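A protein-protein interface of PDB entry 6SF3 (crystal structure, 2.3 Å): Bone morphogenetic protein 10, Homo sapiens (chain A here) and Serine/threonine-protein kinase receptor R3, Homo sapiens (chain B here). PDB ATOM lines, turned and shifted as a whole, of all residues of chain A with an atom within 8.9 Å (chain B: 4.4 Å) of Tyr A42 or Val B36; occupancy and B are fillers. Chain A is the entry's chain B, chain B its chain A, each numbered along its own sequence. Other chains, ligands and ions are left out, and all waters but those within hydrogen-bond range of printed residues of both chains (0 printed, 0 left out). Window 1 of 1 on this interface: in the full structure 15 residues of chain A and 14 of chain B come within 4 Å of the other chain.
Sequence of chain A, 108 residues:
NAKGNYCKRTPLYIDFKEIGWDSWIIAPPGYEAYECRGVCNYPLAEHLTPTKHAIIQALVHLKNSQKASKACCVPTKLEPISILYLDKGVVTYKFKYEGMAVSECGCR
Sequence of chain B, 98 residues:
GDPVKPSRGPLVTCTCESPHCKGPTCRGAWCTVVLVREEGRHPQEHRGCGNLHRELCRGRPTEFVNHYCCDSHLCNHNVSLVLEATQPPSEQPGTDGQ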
ATOM      1  N   TYR A   6      24.505  27.592  17.732  1.00  0.00           N
ATOM      2  CA  TYR A   6      24.012  26.283  18.119  1.00  0.00           C
ATOM      3  C   TYR A   6      24.289  25.241  17.039  1.00  0.00           C
ATOM      4  O   TYR A   6      24.447  25.556  15.857  1.00  0.00           O
ATOM      5  CB  TYR A   6      22.519  26.319  18.409  1.00  0.00           C
ATOM      6  CG  TYR A   6      22.123  25.301  19.441  1.00  0.00           C
ATOM      7  CD1 TYR A   6      22.153  25.620  20.796  1.00  0.00           C
ATOM      8  CD2 TYR A   6      21.739  24.015  19.076  1.00  0.00           C
ATOM      9  CE1 TYR A   6      21.802  24.698  21.758  1.00  0.00           C
ATOM     10  CE2 TYR A   6      21.394  23.085  20.032  1.00  0.00           C
ATOM     11  CZ  TYR A   6      21.423  23.438  21.373  1.00  0.00           C
ATOM     12  OH  TYR A   6      21.070  22.525  22.334  1.00  0.00           O
ATOM     13  N   VAL A  39      27.465  24.437  19.472  1.00  0.00           N
ATOM     14  CA  VAL A  39      27.419  23.853  20.809  1.00  0.00           C
ATOM     15  C   VAL A  39      26.098  23.121  21.018  1.00  0.00           C
ATOM     16  O   VAL A  39      25.065  23.442  20.421  1.00  0.00           O
ATOM     17  CB  VAL A  39      27.623  24.939  21.879  1.00  0.00           C
ATOM     18  CG1 VAL A  39      28.870  25.742  21.570  1.00  0.00           C
ATOM     19  CG2 VAL A  39      26.408  25.833  21.931  1.00  0.00           C
ATOM     20  N   CYS A  40      26.137  22.110  21.879  1.00  0.00           N
ATOM     21  CA  CYS A  40      24.960  21.350  22.273  1.00  0.00           C
ATOM     22  C   CYS A  40      24.659  21.725  23.721  1.00  0.00           C
ATOM     23  O   CYS A  40      25.099  21.063  24.659  1.00  0.00           O
ATOM     24  CB  CYS A  40      25.190  19.839  22.106  1.00  0.00           C
ATOM     25  SG  CYS A  40      25.232  19.247  20.360  1.00  0.00           S
ATOM     26  N   ASN A  41      23.908  22.811  23.898  1.00  0.00           N
ATOM     27  CA  ASN A  41      23.605  23.318  25.234  1.00  0.00           C
ATOM     28  C   ASN A  41      22.284  22.763  25.730  1.00  0.00           C
ATOM     29  O   ASN A  41      21.314  22.661  24.973  1.00  0.00           O
ATOM     30  CB  ASN A  41      23.563  24.846  25.247  1.00  0.00           C
ATOM     31  CG  ASN A  41      24.945  25.462  25.389  1.00  0.00           C
ATOM     32  OD1 ASN A  41      25.825  24.888  26.029  1.00  0.00           O
ATOM     33  ND2 ASN A  41      25.140  26.634  24.795  1.00  0.00           N
ATOM     34  N   TYR A  42      22.252  22.396  27.005  1.00  0.00           N
ATOM     35  CA  TYR A  42      21.000  21.950  27.600  1.00  0.00           C
ATOM     36  C   TYR A  42      19.961  23.069  27.542  1.00  0.00           C
ATOM     37  O   TYR A  42      20.275  24.230  27.837  1.00  0.00           O
ATOM     38  CB  TYR A  42      21.205  21.513  29.044  1.00  0.00           C
ATOM     39  CG  TYR A  42      20.073  20.654  29.506  1.00  0.00           C
ATOM     40  CD1 TYR A  42      20.072  19.289  29.259  1.00  0.00           C
ATOM     41  CD2 TYR A  42      18.975  21.207  30.152  1.00  0.00           C
ATOM     42  CE1 TYR A  42      19.010  18.489  29.666  1.00  0.00           C
ATOM     43  CE2 TYR A  42      17.916  20.423  30.556  1.00  0.00           C
ATOM     44  CZ  TYR A  42      17.937  19.065  30.310  1.00  0.00           C
ATOM     45  OH  TYR A  42      16.879  18.282  30.714  1.00  0.00           O
ATOM     46  N   PRO A  43      18.714  22.768  27.157  1.00  0.00           N
ATOM     47  CA  PRO A  43      18.193  21.443  26.801  1.00  0.00           C
ATOM     48  C   PRO A  43      18.427  21.086  25.322  1.00  0.00           C
ATOM     49  O   PRO A  43      18.457  21.974  24.471  1.00  0.00           O
ATOM     50  CB  PRO A  43      16.706  21.578  27.113  1.00  0.00           C
ATOM     51  CG  PRO A  43      16.408  23.032  26.786  1.00  0.00           C
ATOM     52  CD  PRO A  43      17.663  23.805  27.111  1.00  0.00           C
ATOM     53  N   LEU A  44      18.593  19.796  25.039  1.00  0.00           N
ATOM     54  CA  LEU A  44      18.987  19.332  23.712  1.00  0.00           C
ATOM     55  C   LEU A  44      17.740  19.199  22.847  1.00  0.00           C
ATOM     56  O   LEU A  44      16.906  18.320  23.092  1.00  0.00           O
ATOM     57  CB  LEU A  44      19.740  18.005  23.808  1.00  0.00           C
ATOM     58  CG  LEU A  44      20.971  17.944  24.732  1.00  0.00           C
ATOM     59  CD1 LEU A  44      21.579  16.518  24.809  1.00  0.00           C
ATOM     60  CD2 LEU A  44      22.039  18.968  24.343  1.00  0.00           C
ATOM     61  N   ALA A  45      17.626  20.056  21.832  1.00  0.00           N
ATOM     62  CA  ALA A  45      16.443  20.090  20.976  1.00  0.00           C
ATOM     63  C   ALA A  45      16.181  18.725  20.366  1.00  0.00           C
ATOM     64  O   ALA A  45      17.111  17.978  20.049  1.00  0.00           O
ATOM     65  CB  ALA A  45      16.624  21.122  19.862  1.00  0.00           C
ATOM     66  N   PRO A  50      18.843  13.761  20.422  1.00  0.00           N
ATOM     67  CA  PRO A  50      19.760  13.354  21.493  1.00  0.00           C
ATOM     68  C   PRO A  50      19.420  11.968  22.019  1.00  0.00           C
ATOM     69  O   PRO A  50      18.257  11.568  22.071  1.00  0.00           O
ATOM     70  CB  PRO A  50      19.545  14.427  22.574  1.00  0.00           C
ATOM     71  CG  PRO A  50      18.123  14.876  22.360  1.00  0.00           C
ATOM     72  CD  PRO A  50      17.907  14.824  20.861  1.00  0.00           C
ATOM     73  N   THR A  51      20.457  11.221  22.373  1.00  0.00           N
ATOM     74  CA  THR A  51      20.308   9.979  23.119  1.00  0.00           C
ATOM     75  C   THR A  51      20.031  10.309  24.580  1.00  0.00           C
ATOM     76  O   THR A  51      20.240  11.437  25.034  1.00  0.00           O
ATOM     77  CB  THR A  51      21.587   9.142  23.048  1.00  0.00           C
ATOM     78  OG1 THR A  51      22.662   9.911  23.606  1.00  0.00           O
ATOM     79  CG2 THR A  51      21.944   8.732  21.597  1.00  0.00           C
ATOM     80  N   LYS A  52      19.613   9.294  25.335  1.00  0.00           N
ATOM     81  CA  LYS A  52      19.496   9.460  26.781  1.00  0.00           C
ATOM     82  C   LYS A  52      20.853   9.740  27.413  1.00  0.00           C
ATOM     83  O   LYS A  52      20.970  10.579  28.317  1.00  0.00           O
ATOM     84  CB  LYS A  52      18.859   8.215  27.407  1.00  0.00           C
ATOM     85  CG  LYS A  52      17.334   8.127  27.227  1.00  0.00           C
ATOM     86  CD  LYS A  52      16.784   6.883  27.918  1.00  0.00           C
ATOM     87  CE  LYS A  52      15.583   6.312  27.184  1.00  0.00           C
ATOM     88  NZ  LYS A  52      15.675   4.827  27.040  1.00  0.00           N
ATOM     89  N   HIS A  53      21.895   9.050  26.943  1.00  0.00           N
ATOM     90  CA  HIS A  53      23.234   9.301  27.456  1.00  0.00           C
ATOM     91  C   HIS A  53      23.634  10.757  27.241  1.00  0.00           C
ATOM     92  O   HIS A  53      24.144  11.412  28.155  1.00  0.00           O
ATOM     93  CB  HIS A  53      24.248   8.360  26.792  1.00  0.00           C
ATOM     94  CG  HIS A  53      25.612   8.469  27.387  1.00  0.00           C
ATOM     95  ND1 HIS A  53      26.543   9.380  26.942  1.00  0.00           N
ATOM     96  CD2 HIS A  53      26.181   7.827  28.435  1.00  0.00           C
ATOM     97  CE1 HIS A  53      27.640   9.274  27.672  1.00  0.00           C
ATOM     98  NE2 HIS A  53      27.448   8.337  28.583  1.00  0.00           N
ATOM     99  N   ALA A  54      23.420  11.282  26.032  1.00  0.00           N
ATOM    100  CA  ALA A  54      23.768  12.677  25.781  1.00  0.00           C
ATOM    101  C   ALA A  54      23.001  13.618  26.713  1.00  0.00           C
ATOM    102  O   ALA A  54      23.579  14.568  27.256  1.00  0.00           O
ATOM    103  CB  ALA A  54      23.516  13.029  24.314  1.00  0.00           C
ATOM    104  N   ILE A  55      21.715  13.341  26.948  1.00  0.00           N
ATOM    105  CA  ILE A  55      20.913  14.191  27.832  1.00  0.00           C
ATOM    106  C   ILE A  55      21.451  14.135  29.254  1.00  0.00           C
ATOM    107  O   ILE A  55      21.644  15.168  29.910  1.00  0.00           O
ATOM    108  CB  ILE A  55      19.429  13.784  27.768  1.00  0.00           C
ATOM    109  CG1 ILE A  55      18.852  14.169  26.411  1.00  0.00           C
ATOM    110  CG2 ILE A  55      18.621  14.470  28.884  1.00  0.00           C
ATOM    111  CD1 ILE A  55      17.625  13.408  26.051  1.00  0.00           C
ATOM    112  N   ILE A  56      21.727  12.927  29.740  1.00  0.00           N
ATOM    113  CA  ILE A  56      22.260  12.777  31.091  1.00  0.00           C
ATOM    114  C   ILE A  56      23.624  13.449  31.206  1.00  0.00           C
ATOM    115  O   ILE A  56      23.899  14.175  32.168  1.00  0.00           O
ATOM    116  CB  ILE A  56      22.325  11.283  31.460  1.00  0.00           C
ATOM    117  CG1 ILE A  56      20.926  10.778  31.787  1.00  0.00           C
ATOM    118  CG2 ILE A  56      23.257  11.052  32.638  1.00  0.00           C
ATOM    119  CD1 ILE A  56      20.869   9.306  32.014  1.00  0.00           C
ATOM    120  N   GLN A  57      24.497  13.229  30.222  1.00  0.00           N
ATOM    121  CA  GLN A  57      25.802  13.872  30.267  1.00  0.00           C
ATOM    122  C   GLN A  57      25.665  15.389  30.227  1.00  0.00           C
ATOM    123  O   GLN A  57      26.343  16.097  30.978  1.00  0.00           O
ATOM    124  CB  GLN A  57      26.685  13.368  29.123  1.00  0.00           C
ATOM    125  CG  GLN A  57      27.980  14.116  29.026  1.00  0.00           C
ATOM    126  CD  GLN A  57      28.964  13.487  28.057  1.00  0.00           C
ATOM    127  OE1 GLN A  57      28.632  12.565  27.315  1.00  0.00           O
ATOM    128  NE2 GLN A  57      30.195  13.977  28.078  1.00  0.00           N
ATOM    129  N   ALA A  58      24.792  15.907  29.358  1.00  0.00           N
ATOM    130  CA  ALA A  58      24.535  17.345  29.357  1.00  0.00           C
ATOM    131  C   ALA A  58      24.095  17.829  30.733  1.00  0.00           C
ATOM    132  O   ALA A  58      24.530  18.889  31.192  1.00  0.00           O
ATOM    133  CB  ALA A  58      23.485  17.685  28.309  1.00  0.00           C
ATOM    134  N   LEU A  59      23.249  17.052  31.420  1.00  0.00           N
ATOM    135  CA  LEU A  59      22.802  17.441  32.758  1.00  0.00           C
ATOM    136  C   LEU A  59      23.947  17.445  33.767  1.00  0.00           C
ATOM    137  O   LEU A  59      24.045  18.356  34.596  1.00  0.00           O
ATOM    138  CB  LEU A  59      21.681  16.517  33.230  1.00  0.00           C
ATOM    139  CG  LEU A  59      20.291  16.833  32.675  1.00  0.00           C
ATOM    140  CD1 LEU A  59      19.351  15.691  32.929  1.00  0.00           C
ATOM    141  CD2 LEU A  59      19.782  18.085  33.331  1.00  0.00           C
ATOM    142  N   VAL A  60      24.814  16.433  33.732  1.00  0.00           N
ATOM    143  CA  VAL A  60      25.937  16.407  34.667  1.00  0.00           C
ATOM    144  C   VAL A  60      26.881  17.573  34.394  1.00  0.00           C
ATOM    145  O   VAL A  60      27.392  18.208  35.326  1.00  0.00           O
ATOM    146  CB  VAL A  60      26.671  15.057  34.588  1.00  0.00           C
ATOM    147  CG1 VAL A  60      27.943  15.101  35.416  1.00  0.00           C
ATOM    148  CG2 VAL A  60      25.773  13.967  35.088  1.00  0.00           C
ATOM    149  N   HIS A  61      27.128  17.868  33.113  1.00  0.00           N
ATOM    150  CA  HIS A  61      28.010  18.977  32.766  1.00  0.00           C
ATOM    151  C   HIS A  61      27.468  20.292  33.298  1.00  0.00           C
ATOM    152  O   HIS A  61      28.235  21.148  33.754  1.00  0.00           O
ATOM    153  CB  HIS A  61      28.191  19.071  31.253  1.00  0.00           C
ATOM    154  CG  HIS A  61      28.864  20.336  30.825  1.00  0.00           C
ATOM    155  ND1 HIS A  61      30.237  20.464  30.765  1.00  0.00           N
ATOM    156  CD2 HIS A  61      28.357  21.548  30.499  1.00  0.00           C
ATOM    157  CE1 HIS A  61      30.544  21.692  30.391  1.00  0.00           C
ATOM    158  NE2 HIS A  61      29.423  22.370  30.223  1.00  0.00           N
ATOM    159  N   LEU A  62      26.147  20.471  33.227  1.00  0.00           N
ATOM    160  CA  LEU A  62      25.503  21.648  33.799  1.00  0.00           C
ATOM    161  C   LEU A  62      25.806  21.782  35.284  1.00  0.00           C
ATOM    162  O   LEU A  62      26.081  22.883  35.775  1.00  0.00           O
ATOM    163  CB  LEU A  62      24.000  21.545  33.580  1.00  0.00           C
ATOM    164  CG  LEU A  62      23.241  22.751  33.084  1.00  0.00           C
ATOM    165  CD1 LEU A  62      23.826  23.179  31.763  1.00  0.00           C
ATOM    166  CD2 LEU A  62      21.783  22.342  32.953  1.00  0.00           C
ATOM    167  N   LYS A  63      25.749  20.670  36.017  1.00  0.00           N
ATOM    168  CA  LYS A  63      26.007  20.707  37.452  1.00  0.00           C
ATOM    169  C   LYS A  63      27.482  20.897  37.759  1.00  0.00           C
ATOM    170  O   LYS A  63      27.828  21.572  38.728  1.00  0.00           O
ATOM    171  CB  LYS A  63      25.492  19.427  38.110  1.00  0.00           C
ATOM    172  CG  LYS A  63      26.075  19.153  39.488  1.00  0.00           C
ATOM    173  CD  LYS A  63      25.262  18.100  40.222  1.00  0.00           C
ATOM    174  CE  LYS A  63      25.839  17.814  41.606  1.00  0.00           C
ATOM    175  NZ  LYS A  63      25.780  18.983  42.535  1.00  0.00           N
ATOM    176  N   LYS A  70      30.431  18.765  27.571  1.00  0.00           N
ATOM    177  CA  LYS A  70      29.174  18.930  26.857  1.00  0.00           C
ATOM    178  C   LYS A  70      28.987  17.804  25.851  1.00  0.00           C
ATOM    179  O   LYS A  70      29.946  17.180  25.391  1.00  0.00           O
ATOM    180  CB  LYS A  70      29.130  20.278  26.134  1.00  0.00           C
ATOM    181  CG  LYS A  70      28.913  21.479  27.044  1.00  0.00           C
ATOM    182  CD  LYS A  70      28.722  22.747  26.229  1.00  0.00           C
ATOM    183  CE  LYS A  70      28.771  23.987  27.111  1.00  0.00           C
ATOM    184  NZ  LYS A  70      28.745  25.243  26.310  1.00  0.00           N
ATOM    185  N   ALA A  71      27.732  17.534  25.513  1.00  0.00           N
ATOM    186  CA  ALA A  71      27.482  16.687  24.360  1.00  0.00           C
ATOM    187  C   ALA A  71      28.016  17.373  23.099  1.00  0.00           C
ATOM    188  O   ALA A  71      28.234  18.590  23.061  1.00  0.00           O
ATOM    189  CB  ALA A  71      25.991  16.369  24.235  1.00  0.00           C
ATOM    190  N   CYS A 107      23.191  15.696  18.268  1.00  0.00           N
ATOM    191  CA  CYS A 107      23.958  15.851  19.499  1.00  0.00           C
ATOM    192  C   CYS A 107      24.134  14.477  20.126  1.00  0.00           C
ATOM    193  O   CYS A 107      23.156  13.744  20.313  1.00  0.00           O
ATOM    194  CB  CYS A 107      23.280  16.811  20.489  1.00  0.00           C
ATOM    195  SG  CYS A 107      23.316  18.582  20.029  1.00  0.00           S
ATOM    196  N   VAL B  34      11.618  25.186  30.350  1.00  0.00           N
ATOM    197  CA  VAL B  34      12.842  24.675  30.945  1.00  0.00           C
ATOM    198  C   VAL B  34      13.646  25.866  31.403  1.00  0.00           C
ATOM    199  O   VAL B  34      13.950  26.757  30.598  1.00  0.00           O
ATOM    200  CB  VAL B  34      13.675  23.819  29.970  1.00  0.00           C
ATOM    201  CG1 VAL B  34      14.936  23.324  30.674  1.00  0.00           C
ATOM    202  CG2 VAL B  34      12.865  22.638  29.469  1.00  0.00           C
ATOM    203  N   LEU B  35      13.977  25.893  32.688  1.00  0.00           N
ATOM    204  CA  LEU B  35      14.839  26.918  33.259  1.00  0.00           C
ATOM    205  C   LEU B  35      16.196  26.297  33.532  1.00  0.00           C
ATOM    206  O   LEU B  35      16.280  25.291  34.244  1.00  0.00           O
ATOM    207  CB  LEU B  35      14.253  27.469  34.551  1.00  0.00           C
ATOM    208  CG  LEU B  35      14.929  28.691  35.164  1.00  0.00           C
ATOM    209  CD1 LEU B  35      15.023  29.821  34.156  1.00  0.00           C
ATOM    210  CD2 LEU B  35      14.119  29.127  36.403  1.00  0.00           C
ATOM    211  N   VAL B  36      17.243  26.906  32.984  1.00  0.00           N
ATOM    212  CA  VAL B  36      18.593  26.355  33.007  1.00  0.00           C
ATOM    213  C   VAL B  36      19.546  27.406  33.546  1.00  0.00           C
ATOM    214  O   VAL B  36      19.599  28.524  33.027  1.00  0.00           O
ATOM    215  CB  VAL B  36      19.061  25.909  31.606  1.00  0.00           C
ATOM    216  CG1 VAL B  36      20.495  25.442  31.672  1.00  0.00           C
ATOM    217  CG2 VAL B  36      18.203  24.805  31.091  1.00  0.00           C
ATOM    218  N   ARG B  37      20.327  27.034  34.553  1.00  0.00           N
ATOM    219  CA  ARG B  37      21.458  27.836  35.011  1.00  0.00           C
ATOM    220  C   ARG B  37      22.766  27.101  34.723  1.00  0.00           C
ATOM    221  O   ARG B  37      23.127  26.169  35.444  1.00  0.00           O
ATOM    222  CB  ARG B  37      21.333  28.124  36.486  1.00  0.00           C
ATOM    223  CG  ARG B  37      22.480  28.896  37.033  1.00  0.00           C
ATOM    224  CD  ARG B  37      22.098  29.448  38.386  1.00  0.00           C
ATOM    225  NE  ARG B  37      22.994  30.532  38.744  1.00  0.00           N
ATOM    226  CZ  ARG B  37      22.768  31.390  39.726  1.00  0.00           C
ATOM    227  NH1 ARG B  37      21.659  31.288  40.449  1.00  0.00           N
ATOM    228  NH2 ARG B  37      23.652  32.346  39.976  1.00  0.00           N
ATOM    229  N   GLU B  38      23.484  27.527  33.686  1.00  0.00           N
ATOM    230  CA  GLU B  38      24.839  27.030  33.463  1.00  0.00           C
ATOM    231  C   GLU B  38      25.828  27.799  34.331  1.00  0.00           C
ATOM    232  O   GLU B  38      25.656  28.995  34.577  1.00  0.00           O
ATOM    233  CB  GLU B  38      25.236  27.136  31.990  1.00  0.00           C
ATOM    234  CG  GLU B  38      26.620  26.538  31.700  1.00  0.00           C
ATOM    235  CD  GLU B  38      26.800  26.028  30.271  1.00  0.00           C
ATOM    236  OE1 GLU B  38      25.784  25.766  29.591  1.00  0.00           O
ATOM    237  OE2 GLU B  38      27.967  25.884  29.835  1.00  0.00           O
ATOM    238  N   HIS B  42      23.532  33.568  34.265  1.00  0.00           N
ATOM    239  CA  HIS B  42      22.190  33.847  34.746  1.00  0.00           C
ATOM    240  C   HIS B  42      21.206  32.829  34.178  1.00  0.00           C
ATOM    241  O   HIS B  42      21.339  32.427  33.017  1.00  0.00           O
ATOM    242  CB  HIS B  42      21.767  35.249  34.336  1.00  0.00           C
ATOM    243  CG  HIS B  42      20.567  35.744  35.070  1.00  0.00           C
ATOM    244  ND1 HIS B  42      20.569  35.959  36.433  1.00  0.00           N
ATOM    245  CD2 HIS B  42      19.316  36.028  34.644  1.00  0.00           C
ATOM    246  CE1 HIS B  42      19.372  36.364  36.812  1.00  0.00           C
ATOM    247  NE2 HIS B  42      18.596  36.425  35.744  1.00  0.00           N
ATOM    248  N   PRO B  43      20.216  32.387  34.964  1.00  0.00           N
ATOM    249  CA  PRO B  43      19.299  31.350  34.473  1.00  0.00           C
ATOM    250  C   PRO B  43      18.570  31.811  33.224  1.00  0.00           C
ATOM    251  O   PRO B  43      18.131  32.958  33.126  1.00  0.00           O
ATOM    252  CB  PRO B  43      18.331  31.148  35.640  1.00  0.00           C
ATOM    253  CG  PRO B  43      19.013  31.728  36.825  1.00  0.00           C
ATOM    254  CD  PRO B  43      19.856  32.834  36.318  1.00  0.00           C
ATOM    255  N   GLN B  44      18.443  30.899  32.267  1.00  0.00           N
ATOM    256  CA  GLN B  44      17.827  31.169  30.977  1.00  0.00           C
ATOM    257  C   GLN B  44      16.593  30.288  30.799  1.00  0.00           C
ATOM    258  O   GLN B  44      16.619  29.095  31.109  1.00  0.00           O
ATOM    259  CB  GLN B  44      18.834  30.928  29.854  1.00  0.00           C
ATOM    260  CG  GLN B  44      18.388  31.348  28.469  1.00  0.00           C
ATOM    261  CD  GLN B  44      19.426  30.991  27.412  1.00  0.00           C
ATOM    262  OE1 GLN B  44      20.597  30.767  27.731  1.00  0.00           O
ATOM    263  NE2 GLN B  44      19.000  30.924  26.151  1.00  0.00           N
ATOM    264  N   LEU B  56      11.878  13.652  31.353  1.00  0.00           N
ATOM    265  CA  LEU B  56      12.446  14.927  31.809  1.00  0.00           C
ATOM    266  C   LEU B  56      11.419  15.775  32.558  1.00  0.00           C
ATOM    267  O   LEU B  56      11.772  16.488  33.509  1.00  0.00           O
ATOM    268  CB  LEU B  56      12.987  15.735  30.633  1.00  0.00           C
ATOM    269  CG  LEU B  56      14.186  15.159  29.878  1.00  0.00           C
ATOM    270  CD1 LEU B  56      14.542  16.059  28.701  1.00  0.00           C
ATOM    271  CD2 LEU B  56      15.394  14.958  30.811  1.00  0.00           C
ATOM    272  N   PHE B  64      20.342  23.751  39.217  1.00  0.00           N
ATOM    273  CA  PHE B  64      20.772  24.155  37.899  1.00  0.00           C
ATOM    274  C   PHE B  64      19.721  23.958  36.820  1.00  0.00           C
ATOM    275  O   PHE B  64      19.903  24.486  35.717  1.00  0.00           O
ATOM    276  CB  PHE B  64      22.064  23.417  37.508  1.00  0.00           C
ATOM    277  CG  PHE B  64      21.982  21.941  37.697  1.00  0.00           C
ATOM    278  CD1 PHE B  64      22.254  21.375  38.932  1.00  0.00           C
ATOM    279  CD2 PHE B  64      21.609  21.112  36.643  1.00  0.00           C
ATOM    280  CE1 PHE B  64      22.159  20.012  39.118  1.00  0.00           C
ATOM    281  CE2 PHE B  64      21.518  19.742  36.818  1.00  0.00           C
ATOM    282  CZ  PHE B  64      21.794  19.191  38.055  1.00  0.00           C
ATOM    283  N   VAL B  65      18.625  23.249  37.094  1.00  0.00           N
ATOM    284  CA  VAL B  65      17.631  22.995  36.060  1.00  0.00           C
ATOM    285  C   VAL B  65      16.261  22.769  36.696  1.00  0.00           C
ATOM    286  O   VAL B  65      16.144  22.286  37.824  1.00  0.00           O
ATOM    287  CB  VAL B  65      18.045  21.805  35.150  1.00  0.00           C
ATOM    288  CG1 VAL B  65      18.168  20.537  35.950  1.00  0.00           C
ATOM    289  CG2 VAL B  65      17.046  21.606  34.038  1.00  0.00           C
ATOM    290  N   HIS B  67      12.251  21.640  34.984  1.00  0.00           N
ATOM    291  CA  HIS B  67      11.357  21.371  33.866  1.00  0.00           C
ATOM    292  C   HIS B  67       9.904  21.528  34.278  1.00  0.00           C
ATOM    293  O   HIS B  67       9.511  21.121  35.374  1.00  0.00           O
ATOM    294  CB  HIS B  67      11.530  19.960  33.331  1.00  0.00           C
ATOM    295  CG  HIS B  67      12.881  19.695  32.776  1.00  0.00           C
ATOM    296  ND1 HIS B  67      13.968  19.416  33.576  1.00  0.00           N
ATOM    297  CD2 HIS B  67      13.330  19.672  31.500  1.00  0.00           C
ATOM    298  CE1 HIS B  67      15.030  19.227  32.816  1.00  0.00           C
ATOM    299  NE2 HIS B  67      14.671  19.378  31.552  1.00  0.00           N
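NE2 of His B67 sits at hydrogen-bond distance from OH of Tyr A42 (2.6 Å). The side-chain carboxylate of Glu B38 is in salt-bridge range of the side-chain amino group of Lys A70 (3.7 Å).
OD1 of Asn A41 sits at hydrogen-bond distance from NZ of Lys A70, at 3.0 Å. OH of Tyr A6 is in hydrogen-bond range of O of Asn A41. The side-chain sulfur of Cys A40 forms a disulfide with the side-chain sulfur of Cys A107. O of Val B36 lies within hydrogen-bond range of N of Gln B44. N of Arg B37 lies within hydrogen-bond range of O of Phe B64, at 2.8 Å.
Among the printed residues, pairs that only touch across the chains: Asn A41 with Glu B38 (3.7 Å), Tyr A42 with Val B36 (3.8 Å), Tyr A42 with Leu B56 (3.6 Å), Tyr A42 with Val B65 (3.8 Å), Ile A55 with Leu B56 (3.8 Å), Leu A59 with Phe B64 (3.6 Å), Leu A59 with Val B65 (3.9 Å), His A61 with Glu B38 (3.8 Å), Leu A62 with Val B36 (3.6 Å), Leu A62 with Glu B38 (3.9 Å), Leu A62 with Phe B64 (3.9 Å) and Lys A63 with Phe B64 (3.5 Å).
Tyr A42 touches four residues of chain B. Pro A50 touches none of the printed residues of chain B. Printed residues of chain B within 4 Å of Lys A63: Phe B64 (3.5 Å). Of chain A, only Tyr A42 and Leu A62 come within 4 Å of Val B36. Arg B37 touches none of the printed residues of chain A. Printed residues of chain A within 4 Å of Val B65: Tyr A42 (3.8 Å) and Leu A59 (3.9 Å). Printed residues of chain A within 4 Å of His B67: Tyr A42.
Of the 25 printed residues of chain A, 8 touch a printed residue of chain B. Printed residues of chain A that touch a printed residue of chain B: Asn A41, Tyr A42, Ile A55, Leu A59, His A61, Leu A62, Lys A63 and Lys A70. Hydrophobic or aromatic side chains of chain A that line the printed part of chain B: Tyr A42, Ile A55, Leu A59, His A61 and Leu A62. Among the printed residues, Asp or Glu carboxylates within 4 Å of a Lys or Arg side-chain nitrogen of the other chain: Lys A70 with Glu B38 (3.7 Å).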
